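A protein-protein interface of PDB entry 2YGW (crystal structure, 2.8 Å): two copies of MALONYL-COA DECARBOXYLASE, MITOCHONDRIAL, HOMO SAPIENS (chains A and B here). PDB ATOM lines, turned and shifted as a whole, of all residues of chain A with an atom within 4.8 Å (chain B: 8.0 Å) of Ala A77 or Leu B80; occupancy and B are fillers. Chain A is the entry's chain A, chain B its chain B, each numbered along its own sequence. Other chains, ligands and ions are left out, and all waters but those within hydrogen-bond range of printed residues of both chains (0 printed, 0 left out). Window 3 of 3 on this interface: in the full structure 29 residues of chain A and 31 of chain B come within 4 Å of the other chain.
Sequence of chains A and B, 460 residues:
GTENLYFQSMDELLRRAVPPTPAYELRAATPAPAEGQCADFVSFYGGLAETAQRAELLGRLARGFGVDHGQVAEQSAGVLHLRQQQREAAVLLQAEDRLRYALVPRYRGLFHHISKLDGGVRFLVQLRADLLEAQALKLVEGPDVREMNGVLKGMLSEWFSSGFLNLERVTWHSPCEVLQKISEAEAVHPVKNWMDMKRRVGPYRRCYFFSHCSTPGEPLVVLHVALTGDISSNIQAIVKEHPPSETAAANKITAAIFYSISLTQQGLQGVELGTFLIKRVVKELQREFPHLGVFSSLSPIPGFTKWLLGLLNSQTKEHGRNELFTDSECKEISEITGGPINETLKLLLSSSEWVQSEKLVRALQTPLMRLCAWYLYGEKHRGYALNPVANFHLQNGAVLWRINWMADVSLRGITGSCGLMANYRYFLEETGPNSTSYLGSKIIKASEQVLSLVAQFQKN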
ATOM      1  N   ALA A  73     -19.143 -32.211  -8.478  1.00  0.00           N
ATOM      2  CA  ALA A  73     -20.235 -32.067  -7.502  1.00  0.00           C
ATOM      3  C   ALA A  73     -19.721 -32.079  -6.056  1.00  0.00           C
ATOM      4  O   ALA A  73     -20.279 -31.376  -5.207  1.00  0.00           O
ATOM      5  CB  ALA A  73     -21.247 -33.179  -7.695  1.00  0.00           C
ATOM      6  N   GLU A  74     -18.667 -32.888  -5.784  1.00  0.00           N
ATOM      7  CA  GLU A  74     -18.019 -33.005  -4.474  1.00  0.00           C
ATOM      8  C   GLU A  74     -17.305 -31.708  -4.147  1.00  0.00           C
ATOM      9  O   GLU A  74     -17.372 -31.230  -3.013  1.00  0.00           O
ATOM     10  CB  GLU A  74     -17.034 -34.189  -4.454  1.00  0.00           C
ATOM     11  N   GLN A  75     -16.644 -31.132  -5.157  1.00  0.00           N
ATOM     12  CA  GLN A  75     -15.910 -29.875  -5.075  1.00  0.00           C
ATOM     13  C   GLN A  75     -16.843 -28.673  -5.021  1.00  0.00           C
ATOM     14  O   GLN A  75     -16.549 -27.731  -4.283  1.00  0.00           O
ATOM     15  CB  GLN A  75     -14.951 -29.748  -6.240  1.00  0.00           C
ATOM     16  CG  GLN A  75     -13.503 -29.886  -5.802  1.00  0.00           C
ATOM     17  CD  GLN A  75     -13.065 -31.288  -5.461  1.00  0.00           C
ATOM     18  OE1 GLN A  75     -12.623 -31.548  -4.341  1.00  0.00           O
ATOM     19  NE2 GLN A  75     -13.128 -32.196  -6.422  1.00  0.00           N
ATOM     20  N   SER A  76     -17.971 -28.712  -5.783  1.00  0.00           N
ATOM     21  CA  SER A  76     -19.016 -27.678  -5.798  1.00  0.00           C
ATOM     22  C   SER A  76     -19.658 -27.563  -4.403  1.00  0.00           C
ATOM     23  O   SER A  76     -19.854 -26.451  -3.904  1.00  0.00           O
ATOM     24  CB  SER A  76     -20.080 -27.993  -6.848  1.00  0.00           C
ATOM     25  OG  SER A  76     -19.571 -28.031  -8.172  1.00  0.00           O
ATOM     26  N   ALA A  77     -19.947 -28.728  -3.769  1.00  0.00           N
ATOM     27  CA  ALA A  77     -20.511 -28.821  -2.422  1.00  0.00           C
ATOM     28  C   ALA A  77     -19.488 -28.398  -1.371  1.00  0.00           C
ATOM     29  O   ALA A  77     -19.864 -27.754  -0.396  1.00  0.00           O
ATOM     30  CB  ALA A  77     -20.989 -30.234  -2.146  1.00  0.00           C
ATOM     31  N   GLY A  78     -18.215 -28.746  -1.597  1.00  0.00           N
ATOM     32  CA  GLY A  78     -17.088 -28.392  -0.734  1.00  0.00           C
ATOM     33  C   GLY A  78     -16.862 -26.894  -0.612  1.00  0.00           C
ATOM     34  O   GLY A  78     -16.457 -26.419   0.448  1.00  0.00           O
ATOM     35  N   VAL A  79     -17.142 -26.141  -1.702  1.00  0.00           N
ATOM     36  CA  VAL A  79     -17.056 -24.677  -1.778  1.00  0.00           C
ATOM     37  C   VAL A  79     -18.250 -24.091  -1.007  1.00  0.00           C
ATOM     38  O   VAL A  79     -18.067 -23.177  -0.198  1.00  0.00           O
ATOM     39  CB  VAL A  79     -17.003 -24.178  -3.256  1.00  0.00           C
ATOM     40  CG1 VAL A  79     -17.173 -22.665  -3.351  1.00  0.00           C
ATOM     41  CG2 VAL A  79     -15.708 -24.604  -3.928  1.00  0.00           C
ATOM     42  N   LEU A  80     -19.466 -24.644  -1.238  1.00  0.00           N
ATOM     43  CA  LEU A  80     -20.705 -24.215  -0.582  1.00  0.00           C
ATOM     44  C   LEU A  80     -20.701 -24.522   0.920  1.00  0.00           C
ATOM     45  O   LEU A  80     -21.337 -23.792   1.678  1.00  0.00           O
ATOM     46  CB  LEU A  80     -21.925 -24.853  -1.253  1.00  0.00           C
ATOM     47  CG  LEU A  80     -22.344 -24.220  -2.567  1.00  0.00           C
ATOM     48  CD1 LEU A  80     -23.002 -25.221  -3.449  1.00  0.00           C
ATOM     49  CD2 LEU A  80     -23.260 -23.027  -2.348  1.00  0.00           C
ATOM     50  N   HIS A  81     -19.974 -25.579   1.351  1.00  0.00           N
ATOM     51  CA  HIS A  81     -19.839 -25.933   2.760  1.00  0.00           C
ATOM     52  C   HIS A  81     -18.957 -24.902   3.483  1.00  0.00           C
ATOM     53  O   HIS A  81     -19.191 -24.631   4.662  1.00  0.00           O
ATOM     54  CB  HIS A  81     -19.275 -27.348   2.937  1.00  0.00           C
ATOM     55  CG  HIS A  81     -19.025 -27.687   4.369  1.00  0.00           C
ATOM     56  ND1 HIS A  81     -17.752 -27.632   4.909  1.00  0.00           N
ATOM     57  CD2 HIS A  81     -19.909 -27.959   5.358  1.00  0.00           C
ATOM     58  CE1 HIS A  81     -17.895 -27.924   6.193  1.00  0.00           C
ATOM     59  NE2 HIS A  81     -19.175 -28.129   6.510  1.00  0.00           N
ATOM     60  N   ALA B  73     -20.476 -19.672  -6.341  1.00  0.00           N
ATOM     61  CA  ALA B  73     -21.364 -20.375  -5.404  1.00  0.00           C
ATOM     62  C   ALA B  73     -22.761 -20.614  -5.998  1.00  0.00           C
ATOM     63  O   ALA B  73     -23.374 -21.643  -5.709  1.00  0.00           O
ATOM     64  CB  ALA B  73     -21.486 -19.583  -4.119  1.00  0.00           C
ATOM     65  N   GLU B  74     -23.260 -19.657  -6.810  1.00  0.00           N
ATOM     66  CA  GLU B  74     -24.549 -19.741  -7.495  1.00  0.00           C
ATOM     67  C   GLU B  74     -24.492 -20.833  -8.562  1.00  0.00           C
ATOM     68  O   GLU B  74     -25.439 -21.607  -8.714  1.00  0.00           O
ATOM     69  CB  GLU B  74     -24.909 -18.386  -8.140  1.00  0.00           C
ATOM     70  CG  GLU B  74     -25.676 -17.411  -7.252  1.00  0.00           C
ATOM     71  CD  GLU B  74     -26.016 -16.083  -7.916  1.00  0.00           C
ATOM     72  OE1 GLU B  74     -26.552 -16.096  -9.050  1.00  0.00           O
ATOM     73  OE2 GLU B  74     -25.730 -15.026  -7.307  1.00  0.00           O
ATOM     74  N   GLN B  75     -23.369 -20.898  -9.282  1.00  0.00           N
ATOM     75  CA  GLN B  75     -23.092 -21.869 -10.334  1.00  0.00           C
ATOM     76  C   GLN B  75     -22.798 -23.241  -9.753  1.00  0.00           C
ATOM     77  O   GLN B  75     -23.239 -24.226 -10.344  1.00  0.00           O
ATOM     78  CB  GLN B  75     -21.925 -21.394 -11.210  1.00  0.00           C
ATOM     79  CG  GLN B  75     -22.372 -20.985 -12.615  1.00  0.00           C
ATOM     80  CD  GLN B  75     -23.016 -19.630 -12.641  1.00  0.00           C
ATOM     81  OE1 GLN B  75     -22.387 -18.614 -12.356  1.00  0.00           O
ATOM     82  NE2 GLN B  75     -24.279 -19.572 -12.974  1.00  0.00           N
ATOM     83  N   SER B  76     -22.069 -23.306  -8.600  1.00  0.00           N
ATOM     84  CA  SER B  76     -21.742 -24.541  -7.870  1.00  0.00           C
ATOM     85  C   SER B  76     -23.031 -25.207  -7.381  1.00  0.00           C
ATOM     86  O   SER B  76     -23.179 -26.424  -7.520  1.00  0.00           O
ATOM     87  CB  SER B  76     -20.823 -24.256  -6.682  1.00  0.00           C
ATOM     88  OG  SER B  76     -19.572 -23.714  -7.060  1.00  0.00           O
ATOM     89  N   ALA B  77     -23.973 -24.400  -6.828  1.00  0.00           N
ATOM     90  CA  ALA B  77     -25.280 -24.852  -6.349  1.00  0.00           C
ATOM     91  C   ALA B  77     -26.175 -25.267  -7.511  1.00  0.00           C
ATOM     92  O   ALA B  77     -26.902 -26.252  -7.389  1.00  0.00           O
ATOM     93  CB  ALA B  77     -25.951 -23.755  -5.541  1.00  0.00           C
ATOM     94  N   GLY B  78     -26.092 -24.526  -8.619  1.00  0.00           N
ATOM     95  CA  GLY B  78     -26.833 -24.785  -9.850  1.00  0.00           C
ATOM     96  C   GLY B  78     -26.511 -26.129 -10.481  1.00  0.00           C
ATOM     97  O   GLY B  78     -27.396 -26.760 -11.064  1.00  0.00           O
ATOM     98  N   VAL B  79     -25.236 -26.577 -10.355  1.00  0.00           N
ATOM     99  CA  VAL B  79     -24.730 -27.868 -10.840  1.00  0.00           C
ATOM    100  C   VAL B  79     -25.260 -28.972  -9.900  1.00  0.00           C
ATOM    101  O   VAL B  79     -25.762 -29.995 -10.380  1.00  0.00           O
ATOM    102  CB  VAL B  79     -23.178 -27.876 -10.960  1.00  0.00           C
ATOM    103  CG1 VAL B  79     -22.640 -29.280 -11.214  1.00  0.00           C
ATOM    104  CG2 VAL B  79     -22.704 -26.924 -12.052  1.00  0.00           C
ATOM    105  N   LEU B  80     -25.184 -28.736  -8.570  1.00  0.00           N
ATOM    106  CA  LEU B  80     -25.649 -29.668  -7.540  1.00  0.00           C
ATOM    107  C   LEU B  80     -27.174 -29.831  -7.554  1.00  0.00           C
ATOM    108  O   LEU B  80     -27.663 -30.904  -7.192  1.00  0.00           O
ATOM    109  CB  LEU B  80     -25.175 -29.239  -6.157  1.00  0.00           C
ATOM    110  CG  LEU B  80     -23.719 -29.549  -5.842  1.00  0.00           C
ATOM    111  CD1 LEU B  80     -23.183 -28.569  -4.873  1.00  0.00           C
ATOM    112  CD2 LEU B  80     -23.558 -30.946  -5.287  1.00  0.00           C
ATOM    113  N   HIS B  81     -27.922 -28.792  -7.998  1.00  0.00           N
ATOM    114  CA  HIS B  81     -29.383 -28.854  -8.137  1.00  0.00           C
ATOM    115  C   HIS B  81     -29.743 -29.765  -9.324  1.00  0.00           C
ATOM    116  O   HIS B  81     -30.781 -30.422  -9.289  1.00  0.00           O
ATOM    117  CB  HIS B  81     -29.985 -27.453  -8.311  1.00  0.00           C
ATOM    118  N   LEU B  82     -28.842 -29.836 -10.346  1.00  0.00           N
ATOM    119  CA  LEU B  82     -28.959 -30.655 -11.565  1.00  0.00           C
ATOM    120  C   LEU B  82     -28.396 -32.086 -11.383  1.00  0.00           C
ATOM    121  O   LEU B  82     -28.413 -32.878 -12.326  1.00  0.00           O
ATOM    122  CB  LEU B  82     -28.254 -29.969 -12.750  1.00  0.00           C
ATOM    123  CG  LEU B  82     -28.888 -28.687 -13.290  1.00  0.00           C
ATOM    124  CD1 LEU B  82     -27.959 -27.988 -14.219  1.00  0.00           C
ATOM    125  CD2 LEU B  82     -30.185 -28.958 -14.009  1.00  0.00           C
ATOM    126  N   ARG B  83     -27.903 -32.407 -10.180  1.00  0.00           N
ATOM    127  CA  ARG B  83     -27.402 -33.732  -9.810  1.00  0.00           C
ATOM    128  C   ARG B  83     -28.489 -34.535  -9.092  1.00  0.00           C
ATOM    129  O   ARG B  83     -28.617 -35.733  -9.341  1.00  0.00           O
ATOM    130  CB  ARG B  83     -26.164 -33.619  -8.912  1.00  0.00           C
ATOM    131  CG  ARG B  83     -25.424 -34.944  -8.720  1.00  0.00           C
ATOM    132  CD  ARG B  83     -23.951 -34.778  -9.001  1.00  0.00           C
ATOM    133  NE  ARG B  83     -23.260 -36.049  -9.221  1.00  0.00           N
ATOM    134  CZ  ARG B  83     -22.772 -36.441 -10.395  1.00  0.00           C
ATOM    135  NH1 ARG B  83     -22.902 -35.669 -11.469  1.00  0.00           N
ATOM    136  NH2 ARG B  83     -22.149 -37.607 -10.506  1.00  0.00           N
ATOM    137  N   GLN B  84     -29.236 -33.869  -8.165  1.00  0.00           N
ATOM    138  CA  GLN B  84     -30.344 -34.430  -7.375  1.00  0.00           C
ATOM    139  C   GLN B  84     -31.423 -34.974  -8.302  1.00  0.00           C
ATOM    140  O   GLN B  84     -32.088 -35.962  -7.975  1.00  0.00           O
ATOM    141  CB  GLN B  84     -30.935 -33.367  -6.436  1.00  0.00           C
ATOM    142  N   GLN B  85     -31.581 -34.317  -9.464  1.00  0.00           N
ATOM    143  CA  GLN B  85     -32.480 -34.698 -10.540  1.00  0.00           C
ATOM    144  C   GLN B  85     -31.631 -35.007 -11.768  1.00  0.00           C
ATOM    145  O   GLN B  85     -30.899 -34.136 -12.247  1.00  0.00           O
ATOM    146  CB  GLN B  85     -33.554 -33.620 -10.824  1.00  0.00           C
ATOM    147  CG  GLN B  85     -33.067 -32.165 -10.860  1.00  0.00           C
ATOM    148  CD  GLN B  85     -34.080 -31.211 -11.452  1.00  0.00           C
ATOM    149  OE1 GLN B  85     -33.848 -30.602 -12.501  1.00  0.00           O
ATOM    150  NE2 GLN B  85     -35.214 -31.030 -10.781  1.00  0.00           N
ATOM    151  N   LEU B  92     -26.513 -30.282 -18.172  1.00  0.00           N
ATOM    152  CA  LEU B  92     -25.474 -30.308 -17.145  1.00  0.00           C
ATOM    153  C   LEU B  92     -24.203 -29.665 -17.663  1.00  0.00           C
ATOM    154  O   LEU B  92     -23.669 -28.792 -16.980  1.00  0.00           O
ATOM    155  CB  LEU B  92     -25.180 -31.742 -16.641  1.00  0.00           C
ATOM    156  CG  LEU B  92     -23.902 -31.918 -15.783  1.00  0.00           C
ATOM    157  CD1 LEU B  92     -24.174 -31.681 -14.312  1.00  0.00           C
ATOM    158  CD2 LEU B  92     -23.262 -33.269 -16.009  1.00  0.00           C
ATOM    159  N   ALA B  95     -24.104 -25.918 -17.689  1.00  0.00           N
ATOM    160  CA  ALA B  95     -24.073 -25.413 -16.313  1.00  0.00           C
ATOM    161  C   ALA B  95     -22.669 -25.536 -15.731  1.00  0.00           C
ATOM    162  O   ALA B  95     -22.219 -24.631 -15.019  1.00  0.00           O
ATOM    163  CB  ALA B  95     -25.084 -26.162 -15.454  1.00  0.00           C
ATOM    164  N   LEU B  99     -19.951 -22.430 -14.660  1.00  0.00           N
ATOM    165  CA  LEU B  99     -19.107 -22.492 -13.451  1.00  0.00           C
ATOM    166  C   LEU B  99     -17.607 -22.405 -13.822  1.00  0.00           C
ATOM    167  O   LEU B  99     -16.850 -21.724 -13.126  1.00  0.00           O
ATOM    168  CB  LEU B  99     -19.398 -23.793 -12.670  1.00  0.00           C
ATOM    169  CG  LEU B  99     -18.475 -24.161 -11.508  1.00  0.00           C
ATOM    170  CD1 LEU B  99     -18.544 -23.130 -10.383  1.00  0.00           C
ATOM    171  CD2 LEU B  99     -18.807 -25.530 -10.999  1.00  0.00           C
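Among the printed residues, merely in contact across the chains: Ala A73 with Leu B80 (3.3 Å), Ala A73 with Arg B83 (3.4 Å), Ser A76 with Ser B76 (3.5 Å), Ser A76 with Leu B80 (3.7 Å), Ser A76 with Leu B99 (3.9 Å), Ala A77 with Leu B80 (3.4 Å), Leu A80 with Ala B73 (3.6 Å), Leu A80 with Ser B76 (3.9 Å), Leu A80 with Ala B77 (3.6 Å) and Leu A80 with Leu B80 (3.6 Å).
Printed residues of chain A that touch a printed residue of chain B: Ala A73, Ser A76, Ala A77 and Leu A80. Hydrophobic or aromatic side chains of chain A that line the printed part of chain B: Ala A73, Ala A77 and Leu A80. Among the printed residues, no Asp or Glu carboxylate lies within 4 Å of a Lys or Arg side-chain nitrogen of the other chain.
Of the printed residues of chain B, Ala A77 touches Leu B80. Leu B80 touches just these residues of chain A: Ala A73, Ser A76, Ala A77 and Leu A80. No residue of chain B comes within 4 Å of Gly A78. Printed residues of chain A within 4 Å of Ser B76: Ser A76 and Leu A80. Of the printed residues of chain A, Arg B83 touches Ala A73. Printed residues of chain A within 4 Å of Ala B77: Leu A80 (3.6 Å). Of the printed residues of chain B, Ser A76 touches Ser B76, Leu B80 and Leu B99. Of the printed residues of chain B, Leu A80 touches Ala B73 (3.6 Å), Ser B76 (3.9 Å), Ala B77 (3.6 Å) and Leu B80 (3.6 Å). The nearest printed residue of chain A that does not touch Leu B80 is Glu A74 (5.3 Å).
Ala A73 touches Leu B80, and with the chains exchanged Leu A80 touches Ala B73. Ser B76 touches its own counterpart, Ser A76. Ser A76 touches Leu B80, and with the chains exchanged Leu A80 touches Ser B76. Ala A77 touches Leu B80, and with the chains exchanged Leu A80 touches Ala B77. Of the 10 pairs that touch across the chains among the printed residues, 8 have their exchanged pair printed and touching as well.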
